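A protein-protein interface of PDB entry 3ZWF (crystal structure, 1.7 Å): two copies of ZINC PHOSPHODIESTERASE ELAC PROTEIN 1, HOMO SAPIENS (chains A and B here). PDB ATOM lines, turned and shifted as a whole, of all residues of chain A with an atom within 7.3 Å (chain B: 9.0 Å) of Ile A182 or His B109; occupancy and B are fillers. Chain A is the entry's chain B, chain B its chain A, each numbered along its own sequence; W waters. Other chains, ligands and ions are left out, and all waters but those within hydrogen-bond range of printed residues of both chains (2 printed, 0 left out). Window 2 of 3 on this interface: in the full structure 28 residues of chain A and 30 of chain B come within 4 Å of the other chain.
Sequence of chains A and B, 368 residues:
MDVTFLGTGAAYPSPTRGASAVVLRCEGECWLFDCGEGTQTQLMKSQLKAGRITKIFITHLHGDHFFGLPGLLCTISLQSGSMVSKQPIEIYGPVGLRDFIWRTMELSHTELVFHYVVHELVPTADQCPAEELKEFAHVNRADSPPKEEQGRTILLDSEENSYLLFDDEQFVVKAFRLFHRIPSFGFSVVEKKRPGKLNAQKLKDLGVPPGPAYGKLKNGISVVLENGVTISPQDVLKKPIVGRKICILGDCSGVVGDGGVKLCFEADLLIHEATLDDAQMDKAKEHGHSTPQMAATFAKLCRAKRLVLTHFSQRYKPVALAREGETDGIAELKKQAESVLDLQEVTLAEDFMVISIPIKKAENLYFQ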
ATOM      1  N   THR A  59     -17.221  15.131  25.647  1.00  0.00           N
ATOM      2  CA  THR A  59     -18.361  14.754  24.820  1.00  0.00           C
ATOM      3  C   THR A  59     -17.980  14.146  23.458  1.00  0.00           C
ATOM      4  O   THR A  59     -18.657  13.254  22.968  1.00  0.00           O
ATOM      5  CB  THR A  59     -19.332  15.933  24.545  1.00  0.00           C
ATOM      6  OG1 THR A  59     -18.599  17.003  23.914  1.00  0.00           O
ATOM      7  CG2 THR A  59     -20.002  16.471  25.838  1.00  0.00           C
ATOM      8  N   HIS A  60     -16.909  14.658  22.853  1.00  0.00           N
ATOM      9  CA  HIS A  60     -16.464  14.249  21.552  1.00  0.00           C
ATOM     10  C   HIS A  60     -15.087  14.818  21.269  1.00  0.00           C
ATOM     11  O   HIS A  60     -14.697  15.819  21.861  1.00  0.00           O
ATOM     12  CB  HIS A  60     -17.436  14.610  20.436  1.00  0.00           C
ATOM     13  CG  HIS A  60     -17.601  16.064  20.123  1.00  0.00           C
ATOM     14  ND1 HIS A  60     -18.136  16.976  21.007  1.00  0.00           N
ATOM     15  CD2 HIS A  60     -17.457  16.720  18.948  1.00  0.00           C
ATOM     16  CE1 HIS A  60     -18.294  18.131  20.394  1.00  0.00           C
ATOM     17  NE2 HIS A  60     -17.884  18.005  19.146  1.00  0.00           N
ATOM     18  N   LEU A  61     -14.407  14.138  20.360  1.00  0.00           N
ATOM     19  CA  LEU A  61     -12.990  14.488  20.067  1.00  0.00           C
ATOM     20  C   LEU A  61     -12.890  15.524  18.936  1.00  0.00           C
ATOM     21  O   LEU A  61     -12.119  15.340  17.969  1.00  0.00           O
ATOM     22  CB  LEU A  61     -12.177  13.237  19.741  1.00  0.00           C
ATOM     23  CG  LEU A  61     -12.017  12.205  20.872  1.00  0.00           C
ATOM     24  CD1 LEU A  61     -11.316  10.906  20.517  1.00  0.00           C
ATOM     25  CD2 LEU A  61     -11.399  12.878  22.070  1.00  0.00           C
ATOM     26  N   HIS A  62     -13.605  16.640  19.086  1.00  0.00           N
ATOM     27  CA  HIS A  62     -13.303  17.855  18.310  1.00  0.00           C
ATOM     28  C   HIS A  62     -12.465  18.748  19.203  1.00  0.00           C
ATOM     29  O   HIS A  62     -12.689  18.800  20.393  1.00  0.00           O
ATOM     30  CB  HIS A  62     -14.560  18.574  17.860  1.00  0.00           C
ATOM     31  CG  HIS A  62     -15.111  18.057  16.579  1.00  0.00           C
ATOM     32  ND1 HIS A  62     -16.402  18.292  16.200  1.00  0.00           N
ATOM     33  CD2 HIS A  62     -14.533  17.366  15.561  1.00  0.00           C
ATOM     34  CE1 HIS A  62     -16.629  17.724  15.030  1.00  0.00           C
ATOM     35  NE2 HIS A  62     -15.510  17.153  14.613  1.00  0.00           N
ATOM     36  N   GLY A  63     -11.506  19.480  18.636  1.00  0.00           N
ATOM     37  CA  GLY A  63     -10.532  20.205  19.440  1.00  0.00           C
ATOM     38  C   GLY A  63     -11.039  21.248  20.427  1.00  0.00           C
ATOM     39  O   GLY A  63     -10.465  21.424  21.510  1.00  0.00           O
ATOM     40  N   PHE A  66     -11.538  19.396  23.733  1.00  0.00           N
ATOM     41  CA  PHE A  66     -10.500  18.677  24.479  1.00  0.00           C
ATOM     42  C   PHE A  66      -9.070  19.203  24.374  1.00  0.00           C
ATOM     43  O   PHE A  66      -8.235  18.733  25.114  1.00  0.00           O
ATOM     44  CB  PHE A  66     -10.518  17.168  24.181  1.00  0.00           C
ATOM     45  CG  PHE A  66      -9.877  16.767  22.906  1.00  0.00           C
ATOM     46  CD1 PHE A  66     -10.570  16.845  21.706  1.00  0.00           C
ATOM     47  CD2 PHE A  66      -8.585  16.206  22.887  1.00  0.00           C
ATOM     48  CE1 PHE A  66      -9.968  16.492  20.531  1.00  0.00           C
ATOM     49  CE2 PHE A  66      -7.977  15.808  21.678  1.00  0.00           C
ATOM     50  CZ  PHE A  66      -8.686  15.946  20.503  1.00  0.00           C
ATOM     51  N   PRO A  94     -14.355   9.604  24.491  1.00  0.00           N
ATOM     52  CA  PRO A  94     -14.316   8.646  23.433  1.00  0.00           C
ATOM     53  C   PRO A  94     -12.992   7.929  23.284  1.00  0.00           C
ATOM     54  O   PRO A  94     -11.932   8.447  23.630  1.00  0.00           O
ATOM     55  CB  PRO A  94     -14.607   9.485  22.187  1.00  0.00           C
ATOM     56  CG  PRO A  94     -15.205  10.749  22.701  1.00  0.00           C
ATOM     57  CD  PRO A  94     -14.632  10.965  24.008  1.00  0.00           C
ATOM     58  N   PRO A 123     -17.986   4.384  20.680  1.00  0.00           N
ATOM     59  CA  PRO A 123     -19.093   4.826  19.868  1.00  0.00           C
ATOM     60  C   PRO A 123     -19.549   3.812  18.834  1.00  0.00           C
ATOM     61  O   PRO A 123     -18.837   2.820  18.540  1.00  0.00           O
ATOM     62  CB  PRO A 123     -18.550   6.062  19.162  1.00  0.00           C
ATOM     63  CG  PRO A 123     -17.093   5.767  18.984  1.00  0.00           C
ATOM     64  CD  PRO A 123     -16.704   4.932  20.191  1.00  0.00           C
ATOM     65  N   THR A 124     -20.683   4.113  18.226  1.00  0.00           N
ATOM     66  CA  THR A 124     -21.165   3.335  17.083  1.00  0.00           C
ATOM     67  C   THR A 124     -21.195   4.190  15.816  1.00  0.00           C
ATOM     68  O   THR A 124     -21.287   5.412  15.869  1.00  0.00           O
ATOM     69  CB  THR A 124     -22.567   2.716  17.369  1.00  0.00           C
ATOM     70  OG1 THR A 124     -23.526   3.776  17.515  1.00  0.00           O
ATOM     71  CG2 THR A 124     -22.513   1.876  18.641  1.00  0.00           C
ATOM     72  N   GLN A 127     -23.596   7.131  14.700  1.00  0.00           N
ATOM     73  CA  GLN A 127     -23.524   8.411  15.389  1.00  0.00           C
ATOM     74  C   GLN A 127     -22.996   9.506  14.487  1.00  0.00           C
ATOM     75  O   GLN A 127     -22.859  10.647  14.930  1.00  0.00           O
ATOM     76  CB  GLN A 127     -22.600   8.326  16.599  1.00  0.00           C
ATOM     77  CG  GLN A 127     -23.211   7.498  17.714  1.00  0.00           C
ATOM     78  CD  GLN A 127     -22.376   7.584  18.965  1.00  0.00           C
ATOM     79  OE1 GLN A 127     -21.694   6.623  19.345  1.00  0.00           O
ATOM     80  NE2 GLN A 127     -22.414   8.755  19.625  1.00  0.00           N
ATOM     81  N   CYS A 128     -22.589   9.165  13.266  1.00  0.00           N
ATOM     82  CA  CYS A 128     -22.088  10.161  12.338  1.00  0.00           C
ATOM     83  C   CYS A 128     -22.331   9.746  10.893  1.00  0.00           C
ATOM     84  O   CYS A 128     -22.764   8.621  10.647  1.00  0.00           O
ATOM     85  CB  CYS A 128     -20.605  10.456  12.634  1.00  0.00           C
ATOM     86  SG  CYS A 128     -19.541   9.089  12.402  1.00  0.00           S
ATOM     87  N   PRO A 129     -22.088  10.650   9.930  1.00  0.00           N
ATOM     88  CA  PRO A 129     -22.479  10.306   8.572  1.00  0.00           C
ATOM     89  C   PRO A 129     -21.646   9.158   7.987  1.00  0.00           C
ATOM     90  O   PRO A 129     -20.527   8.919   8.430  1.00  0.00           O
ATOM     91  CB  PRO A 129     -22.246  11.608   7.801  1.00  0.00           C
ATOM     92  CG  PRO A 129     -22.312  12.681   8.837  1.00  0.00           C
ATOM     93  CD  PRO A 129     -21.675  12.064  10.037  1.00  0.00           C
ATOM     94  N   LEU A 178     -25.222  10.645  20.732  1.00  0.00           N
ATOM     95  CA  LEU A 178     -25.710  11.723  19.899  1.00  0.00           C
ATOM     96  C   LEU A 178     -25.216  11.557  18.482  1.00  0.00           C
ATOM     97  O   LEU A 178     -24.244  10.846  18.222  1.00  0.00           O
ATOM     98  CB  LEU A 178     -25.273  13.074  20.465  1.00  0.00           C
ATOM     99  CG  LEU A 178     -25.580  13.333  21.941  1.00  0.00           C
ATOM    100  CD1 LEU A 178     -24.964  14.681  22.381  1.00  0.00           C
ATOM    101  CD2 LEU A 178     -27.059  13.369  22.206  1.00  0.00           C
ATOM    102  N   PHE A 179     -25.865  12.243  17.557  1.00  0.00           N
ATOM    103  CA  PHE A 179     -25.425  12.318  16.166  1.00  0.00           C
ATOM    104  C   PHE A 179     -24.700  13.653  15.901  1.00  0.00           C
ATOM    105  O   PHE A 179     -25.250  14.714  16.133  1.00  0.00           O
ATOM    106  CB  PHE A 179     -26.610  12.213  15.209  1.00  0.00           C
ATOM    107  CG  PHE A 179     -26.213  11.981  13.795  1.00  0.00           C
ATOM    108  CD1 PHE A 179     -25.893  13.048  12.962  1.00  0.00           C
ATOM    109  CD2 PHE A 179     -26.105  10.671  13.288  1.00  0.00           C
ATOM    110  CE1 PHE A 179     -25.493  12.822  11.650  1.00  0.00           C
ATOM    111  CE2 PHE A 179     -25.713  10.442  11.971  1.00  0.00           C
ATOM    112  CZ  PHE A 179     -25.420  11.515  11.151  1.00  0.00           C
ATOM    113  N   HIS A 180     -23.499  13.576  15.351  1.00  0.00           N
ATOM    114  CA  HIS A 180     -22.700  14.772  15.056  1.00  0.00           C
ATOM    115  C   HIS A 180     -21.783  14.425  13.873  1.00  0.00           C
ATOM    116  O   HIS A 180     -21.877  13.322  13.315  1.00  0.00           O
ATOM    117  CB  HIS A 180     -21.964  15.210  16.335  1.00  0.00           C
ATOM    118  CG  HIS A 180     -21.198  16.504  16.222  1.00  0.00           C
ATOM    119  ND1 HIS A 180     -21.718  17.664  15.681  1.00  0.00           N
ATOM    120  CD2 HIS A 180     -19.914  16.788  16.559  1.00  0.00           C
ATOM    121  CE1 HIS A 180     -20.793  18.617  15.727  1.00  0.00           C
ATOM    122  NE2 HIS A 180     -19.704  18.122  16.287  1.00  0.00           N
ATOM    123  N   ARG A 181     -20.903  15.343  13.473  1.00  0.00           N
ATOM    124  CA  ARG A 181     -19.960  15.072  12.341  1.00  0.00           C
ATOM    125  C   ARG A 181     -19.014  13.947  12.698  1.00  0.00           C
ATOM    126  O   ARG A 181     -18.543  13.219  11.843  1.00  0.00           O
ATOM    127  CB  ARG A 181     -19.139  16.324  11.989  1.00  0.00           C
ATOM    128  CG  ARG A 181     -19.967  17.505  11.517  1.00  0.00           C
ATOM    129  CD  ARG A 181     -19.119  18.560  10.750  1.00  0.00           C
ATOM    130  NE  ARG A 181     -17.899  19.001  11.433  1.00  0.00           N
ATOM    131  CZ  ARG A 181     -17.866  19.708  12.570  1.00  0.00           C
ATOM    132  NH1 ARG A 181     -18.981  20.019  13.228  1.00  0.00           N
ATOM    133  NH2 ARG A 181     -16.696  20.063  13.080  1.00  0.00           N
ATOM    134  N   ILE A 182     -18.689  13.845  13.979  1.00  0.00           N
ATOM    135  CA  ILE A 182     -18.013  12.691  14.550  1.00  0.00           C
ATOM    136  C   ILE A 182     -18.909  12.229  15.692  1.00  0.00           C
ATOM    137  O   ILE A 182     -19.792  12.993  16.118  1.00  0.00           O
ATOM    138  CB  ILE A 182     -16.564  12.974  15.012  1.00  0.00           C
ATOM    139  CG1 ILE A 182     -16.506  13.993  16.133  1.00  0.00           C
ATOM    140  CG2 ILE A 182     -15.691  13.439  13.805  1.00  0.00           C
ATOM    141  CD1 ILE A 182     -15.137  14.076  16.783  1.00  0.00           C
ATOM    142  N   PRO A 183     -18.694  11.012  16.206  1.00  0.00           N
ATOM    143  CA  PRO A 183     -19.545  10.613  17.325  1.00  0.00           C
ATOM    144  C   PRO A 183     -19.419  11.535  18.553  1.00  0.00           C
ATOM    145  O   PRO A 183     -18.327  11.948  18.935  1.00  0.00           O
ATOM    146  CB  PRO A 183     -19.058   9.197  17.654  1.00  0.00           C
ATOM    147  CG  PRO A 183     -18.440   8.713  16.331  1.00  0.00           C
ATOM    148  CD  PRO A 183     -17.779   9.930  15.808  1.00  0.00           C
ATOM    149  N   SER A 184     -20.573  11.768  19.178  1.00  0.00           N
ATOM    150  CA  SER A 184     -20.679  12.679  20.277  1.00  0.00           C
ATOM    151  C   SER A 184     -21.634  12.080  21.314  1.00  0.00           C
ATOM    152  O   SER A 184     -22.512  11.278  20.966  1.00  0.00           O
ATOM    153  CB  SER A 184     -21.160  14.038  19.750  1.00  0.00           C
ATOM    154  OG  SER A 184     -21.296  14.972  20.784  1.00  0.00           O
ATOM    155  N   PHE A 185     -21.427  12.484  22.569  1.00  0.00           N
ATOM    156  CA  PHE A 185     -22.120  11.903  23.706  1.00  0.00           C
ATOM    157  C   PHE A 185     -22.784  12.953  24.538  1.00  0.00           C
ATOM    158  O   PHE A 185     -22.281  14.090  24.643  1.00  0.00           O
ATOM    159  CB  PHE A 185     -21.163  11.093  24.598  1.00  0.00           C
ATOM    160  CG  PHE A 185     -20.531   9.935  23.884  1.00  0.00           C
ATOM    161  CD1 PHE A 185     -21.211   8.742  23.714  1.00  0.00           C
ATOM    162  CD2 PHE A 185     -19.243  10.044  23.405  1.00  0.00           C
ATOM    163  CE1 PHE A 185     -20.638   7.679  23.005  1.00  0.00           C
ATOM    164  CE2 PHE A 185     -18.666   9.009  22.710  1.00  0.00           C
ATOM    165  CZ  PHE A 185     -19.378   7.789  22.532  1.00  0.00           C
ATOM    166  N   ASP A 251     -22.050  18.477  21.170  1.00  0.00           N
ATOM    167  CA  ASP A 251     -22.501  18.953  19.852  1.00  0.00           C
ATOM    168  C   ASP A 251     -23.309  17.859  19.186  1.00  0.00           C
ATOM    169  O   ASP A 251     -22.954  16.679  19.266  1.00  0.00           O
ATOM    170  CB  ASP A 251     -21.329  19.271  18.923  1.00  0.00           C
ATOM    171  CG  ASP A 251     -20.444  20.407  19.417  1.00  0.00           C
ATOM    172  OD1 ASP A 251     -20.664  21.006  20.486  1.00  0.00           O
ATOM    173  OD2 ASP A 251     -19.454  20.655  18.687  1.00  0.00           O
ATOM    174  N   CYS A 252     -24.406  18.256  18.556  1.00  0.00           N
ATOM    175  CA  CYS A 252     -25.304  17.304  17.929  1.00  0.00           C
ATOM    176  C   CYS A 252     -26.324  17.980  17.067  1.00  0.00           C
ATOM    177  O   CYS A 252     -26.660  19.145  17.270  1.00  0.00           O
ATOM    178  CB  CYS A 252     -26.010  16.417  18.971  1.00  0.00           C
ATOM    179  SG  CYS A 252     -27.167  17.250  20.046  1.00  0.00           S
ATOM    180  N   HIS A 287     -23.663  20.575   9.456  1.00  0.00           N
ATOM    181  CA  HIS A 287     -22.451  20.531  10.278  1.00  0.00           C
ATOM    182  C   HIS A 287     -22.631  19.772  11.587  1.00  0.00           C
ATOM    183  O   HIS A 287     -21.785  19.856  12.473  1.00  0.00           O
ATOM    184  CB  HIS A 287     -21.966  21.953  10.558  1.00  0.00           C
ATOM    185  CG  HIS A 287     -21.500  22.670   9.332  1.00  0.00           C
ATOM    186  ND1 HIS A 287     -22.339  23.436   8.554  1.00  0.00           N
ATOM    187  CD2 HIS A 287     -20.284  22.724   8.739  1.00  0.00           C
ATOM    188  CE1 HIS A 287     -21.660  23.937   7.537  1.00  0.00           C
ATOM    189  NE2 HIS A 287     -20.411  23.518   7.625  1.00  0.00           N
ATOM    190  N   GLY A 288     -23.721  19.030  11.699  1.00  0.00           N
ATOM    191  CA  GLY A 288     -24.021  18.213  12.908  1.00  0.00           C
ATOM    192  C   GLY A 288     -24.394  19.036  14.132  1.00  0.00           C
ATOM    193  O   GLY A 288     -24.106  18.669  15.286  1.00  0.00           O
ATOM    194  N   CYS B  74      -5.971  24.762  13.488  1.00  0.00           N
ATOM    195  CA  CYS B  74      -7.399  24.539  13.207  1.00  0.00           C
ATOM    196  C   CYS B  74      -8.115  25.848  12.901  1.00  0.00           C
ATOM    197  O   CYS B  74      -8.883  25.958  11.951  1.00  0.00           O
ATOM    198  CB  CYS B  74      -8.102  23.835  14.377  1.00  0.00           C
ATOM    199  SG  CYS B  74      -7.698  22.163  14.537  1.00  0.00           S
ATOM    200  N   TRP B 102       0.451  15.671  13.471  1.00  0.00           N
ATOM    201  CA  TRP B 102      -0.246  14.764  12.582  1.00  0.00           C
ATOM    202  C   TRP B 102      -1.317  13.977  13.345  1.00  0.00           C
ATOM    203  O   TRP B 102      -2.474  13.871  12.922  1.00  0.00           O
ATOM    204  CB  TRP B 102       0.742  13.767  11.938  1.00  0.00           C
ATOM    205  CG  TRP B 102       0.074  12.775  11.160  1.00  0.00           C
ATOM    206  CD1 TRP B 102      -0.385  11.525  11.591  1.00  0.00           C
ATOM    207  CD2 TRP B 102      -0.335  12.897   9.797  1.00  0.00           C
ATOM    208  NE1 TRP B 102      -1.035  10.896  10.569  1.00  0.00           N
ATOM    209  CE2 TRP B 102      -1.015  11.702   9.455  1.00  0.00           C
ATOM    210  CE3 TRP B 102      -0.187  13.895   8.821  1.00  0.00           C
ATOM    211  CZ2 TRP B 102      -1.535  11.480   8.178  1.00  0.00           C
ATOM    212  CZ3 TRP B 102      -0.707  13.668   7.546  1.00  0.00           C
ATOM    213  CH2 TRP B 102      -1.373  12.471   7.241  1.00  0.00           C
ATOM    214  N   ARG B 103      -0.906  13.412  14.468  1.00  0.00           N
ATOM    215  CA  ARG B 103      -1.796  12.504  15.244  1.00  0.00           C
ATOM    216  C   ARG B 103      -2.948  13.308  15.815  1.00  0.00           C
ATOM    217  O   ARG B 103      -4.100  12.844  15.860  1.00  0.00           O
ATOM    218  CB  ARG B 103      -1.045  11.845  16.398  1.00  0.00           C
ATOM    219  CG  ARG B 103      -0.025  10.772  15.944  1.00  0.00           C
ATOM    220  CD  ARG B 103       0.332   9.855  17.118  1.00  0.00           C
ATOM    221  NE  ARG B 103       1.758   9.548  17.119  1.00  0.00           N
ATOM    222  CZ  ARG B 103       2.379   8.772  16.235  1.00  0.00           C
ATOM    223  NH1 ARG B 103       1.709   8.169  15.254  1.00  0.00           N
ATOM    224  NH2 ARG B 103       3.689   8.594  16.338  1.00  0.00           N
ATOM    225  N   THR B 104      -2.648  14.528  16.262  1.00  0.00           N
ATOM    226  CA  THR B 104      -3.676  15.386  16.891  1.00  0.00           C
ATOM    227  C   THR B 104      -4.726  15.833  15.854  1.00  0.00           C
ATOM    228  O   THR B 104      -5.925  15.829  16.115  1.00  0.00           O
ATOM    229  CB  THR B 104      -3.050  16.565  17.667  1.00  0.00           C
ATOM    230  OG1 THR B 104      -2.122  16.000  18.611  1.00  0.00           O
ATOM    231  CG2 THR B 104      -4.140  17.416  18.416  1.00  0.00           C
ATOM    232  N   MET B 105      -4.267  16.155  14.652  1.00  0.00           N
ATOM    233  CA  MET B 105      -5.184  16.497  13.553  1.00  0.00           C
ATOM    234  C   MET B 105      -6.053  15.290  13.174  1.00  0.00           C
ATOM    235  O   MET B 105      -7.257  15.435  12.933  1.00  0.00           O
ATOM    236  CB  MET B 105      -4.456  17.027  12.331  1.00  0.00           C
ATOM    237  CG  MET B 105      -3.725  18.333  12.564  1.00  0.00           C
ATOM    238  SD  MET B 105      -4.765  19.720  13.006  1.00  0.00           S
ATOM    239  CE  MET B 105      -4.475  19.861  14.765  1.00  0.00           C
ATOM    240  N   GLU B 106      -5.432  14.115  13.104  1.00  0.00           N
ATOM    241  CA  GLU B 106      -6.166  12.888  12.763  1.00  0.00           C
ATOM    242  C   GLU B 106      -7.206  12.587  13.842  1.00  0.00           C
ATOM    243  O   GLU B 106      -8.361  12.264  13.526  1.00  0.00           O
ATOM    244  CB  GLU B 106      -5.210  11.707  12.597  1.00  0.00           C
ATOM    245  CG  GLU B 106      -5.922  10.459  12.144  1.00  0.00           C
ATOM    246  CD  GLU B 106      -5.004   9.279  11.879  1.00  0.00           C
ATOM    247  OE1 GLU B 106      -4.068   9.037  12.674  1.00  0.00           O
ATOM    248  OE2 GLU B 106      -5.253   8.560  10.892  1.00  0.00           O
ATOM    249  N   LEU B 107      -6.780  12.667  15.109  1.00  0.00           N
ATOM    250  CA  LEU B 107      -7.668  12.319  16.255  1.00  0.00           C
ATOM    251  C   LEU B 107      -8.892  13.216  16.271  1.00  0.00           C
ATOM    252  O   LEU B 107     -10.021  12.770  16.635  1.00  0.00           O
ATOM    253  CB  LEU B 107      -6.904  12.418  17.576  1.00  0.00           C
ATOM    254  CG  LEU B 107      -7.630  12.061  18.877  1.00  0.00           C
ATOM    255  CD1 LEU B 107      -7.879  10.539  18.953  1.00  0.00           C
ATOM    256  CD2 LEU B 107      -6.891  12.602  20.116  1.00  0.00           C
ATOM    257  N   SER B 108      -8.691  14.489  15.922  1.00  0.00           N
ATOM    258  CA  SER B 108      -9.774  15.496  15.996  1.00  0.00           C
ATOM    259  C   SER B 108     -10.559  15.607  14.676  1.00  0.00           C
ATOM    260  O   SER B 108     -11.395  16.508  14.526  1.00  0.00           O
ATOM    261  CB  SER B 108      -9.221  16.831  16.415  1.00  0.00           C
ATOM    262  OG  SER B 108      -8.276  17.330  15.493  1.00  0.00           O
ATOM    263  N   HIS B 109     -10.237  14.729  13.731  1.00  0.00           N
ATOM    264  CA  HIS B 109     -10.833  14.716  12.380  1.00  0.00           C
ATOM    265  C   HIS B 109     -10.796  16.091  11.719  1.00  0.00           C
ATOM    266  O   HIS B 109     -11.760  16.570  11.149  1.00  0.00           O
ATOM    267  CB  HIS B 109     -12.284  14.208  12.472  1.00  0.00           C
ATOM    268  CG  HIS B 109     -12.376  12.837  13.034  1.00  0.00           C
ATOM    269  ND1 HIS B 109     -12.606  11.733  12.247  1.00  0.00           N
ATOM    270  CD2 HIS B 109     -12.221  12.376  14.297  1.00  0.00           C
ATOM    271  CE1 HIS B 109     -12.617  10.650  13.003  1.00  0.00           C
ATOM    272  NE2 HIS B 109     -12.396  11.012  14.252  1.00  0.00           N
ATOM    273  N   THR B 110      -9.635  16.717  11.806  1.00  0.00           N
ATOM    274  CA  THR B 110      -9.402  18.001  11.166  1.00  0.00           C
ATOM    275  C   THR B 110      -8.719  17.776   9.825  1.00  0.00           C
ATOM    276  O   THR B 110      -7.642  17.167   9.761  1.00  0.00           O
ATOM    277  CB  THR B 110      -8.481  18.843  12.027  1.00  0.00           C
ATOM    278  OG1 THR B 110      -9.101  19.023  13.293  1.00  0.00           O
ATOM    279  CG2 THR B 110      -8.214  20.209  11.387  1.00  0.00           C
ATOM    280  N   GLU B 111      -9.338  18.290   8.768  1.00  0.00           N
ATOM    281  CA  GLU B 111      -8.713  18.409   7.447  1.00  0.00           C
ATOM    282  C   GLU B 111      -8.373  19.877   7.243  1.00  0.00           C
ATOM    283  O   GLU B 111      -9.245  20.696   6.951  1.00  0.00           O
ATOM    284  CB  GLU B 111      -9.657  17.907   6.334  1.00  0.00           C
ATOM    285  N   LEU B 112      -7.109  20.227   7.448  1.00  0.00           N
ATOM    286  CA  LEU B 112      -6.684  21.626   7.290  1.00  0.00           C
ATOM    287  C   LEU B 112      -6.751  22.010   5.810  1.00  0.00           C
ATOM    288  O   LEU B 112      -6.408  21.214   4.949  1.00  0.00           O
ATOM    289  CB  LEU B 112      -5.277  21.832   7.825  1.00  0.00           C
ATOM    290  CG  LEU B 112      -5.040  21.538   9.315  1.00  0.00           C
ATOM    291  CD1 LEU B 112      -3.545  21.496   9.624  1.00  0.00           C
ATOM    292  CD2 LEU B 112      -5.725  22.529  10.211  1.00  0.00           C
HETATM  293  O   HOH W   1     -15.013  16.481  12.030  1.00  0.00           O
HETATM  294  O   HOH W   2     -11.688  19.292  15.736  1.00  0.00           O
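The side-chain hydroxyl (OG) of Ser B108 lies within hydrogen-bond range of the side-chain hydroxyl (OG1) of Thr B110 (2.9 Å). The backbone carbonyl oxygen (O) of Thr B104 is in hydrogen-bond range of the side-chain hydroxyl (OG) of Ser B108 (2.9 Å). The side-chain hydroxyl (OG) of Ser B108 is in hydrogen-bond range of the backbone carbonyl oxygen (O) of Met B105, 3.3 Å away. A ring nitrogen (NE2) of His A62 lies close to the guanidinium group (NH2) of Arg A181, at 3.5 Å.
O of Leu B107 touches O of Leu A61, 3.6 Å away. Ser B108 touches Leu A61. His A62 touches Ser B108. Phe A66 touches Leu B107 (CE2 to CD2, 3.7 Å). His B109 touches Ile A182.
Ile A182 touches just one residue of chain B: His B109. His B109 touches one residue of chain A. No residue of chain B comes within 4 Å of Pro A183. Of the printed residues of chain A, Ser B108 touches Leu A61 (3.1 Å) and His A62 (3.4 Å). Printed residues of chain B within 4 Å of Phe A66: Leu B107. Cys A128 touches none of the printed residues of chain B. The nearest residue of chain B that does not touch Ile A182 is Ser B108 (5.0 Å). The nearest residue of chain A that does not touch His B109 is Leu A61 (4.7 Å). The nearest printed residue of chain A that does not touch Ser B108 is Gly A63 (4.1 Å).
Of the 12 printed residues of chain B, 3 touch a printed residue of chain A. Printed residues of chain B that touch a printed residue of chain A: Leu B107, Ser B108 and His B109. Of the 24 printed residues of chain A, 4 touch a printed residue of chain B. Printed residues of chain A that touch a printed residue of chain B: Leu A61, His A62, Phe A66 and Ile A182. Along chain A the printed residues that touch a printed residue of chain B span positions 61 to 182. Among the printed residues, no Asp or Glu carboxylate lies within 4 Å of a Lys or Arg side-chain nitrogen of the other chain.
No position is printed for both chains.
Water W1 lies within hydrogen-bond range of a ring nitrogen (NE2) of His A62 (2.7 Å) and the backbone carbonyl oxygen of His B109 (3.4 Å). Water W2 bridges the backbone NH (N) of Gly A63 (2.9 Å) and the backbone carbonyl oxygen (O) of Ser B108 (3.0 Å).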
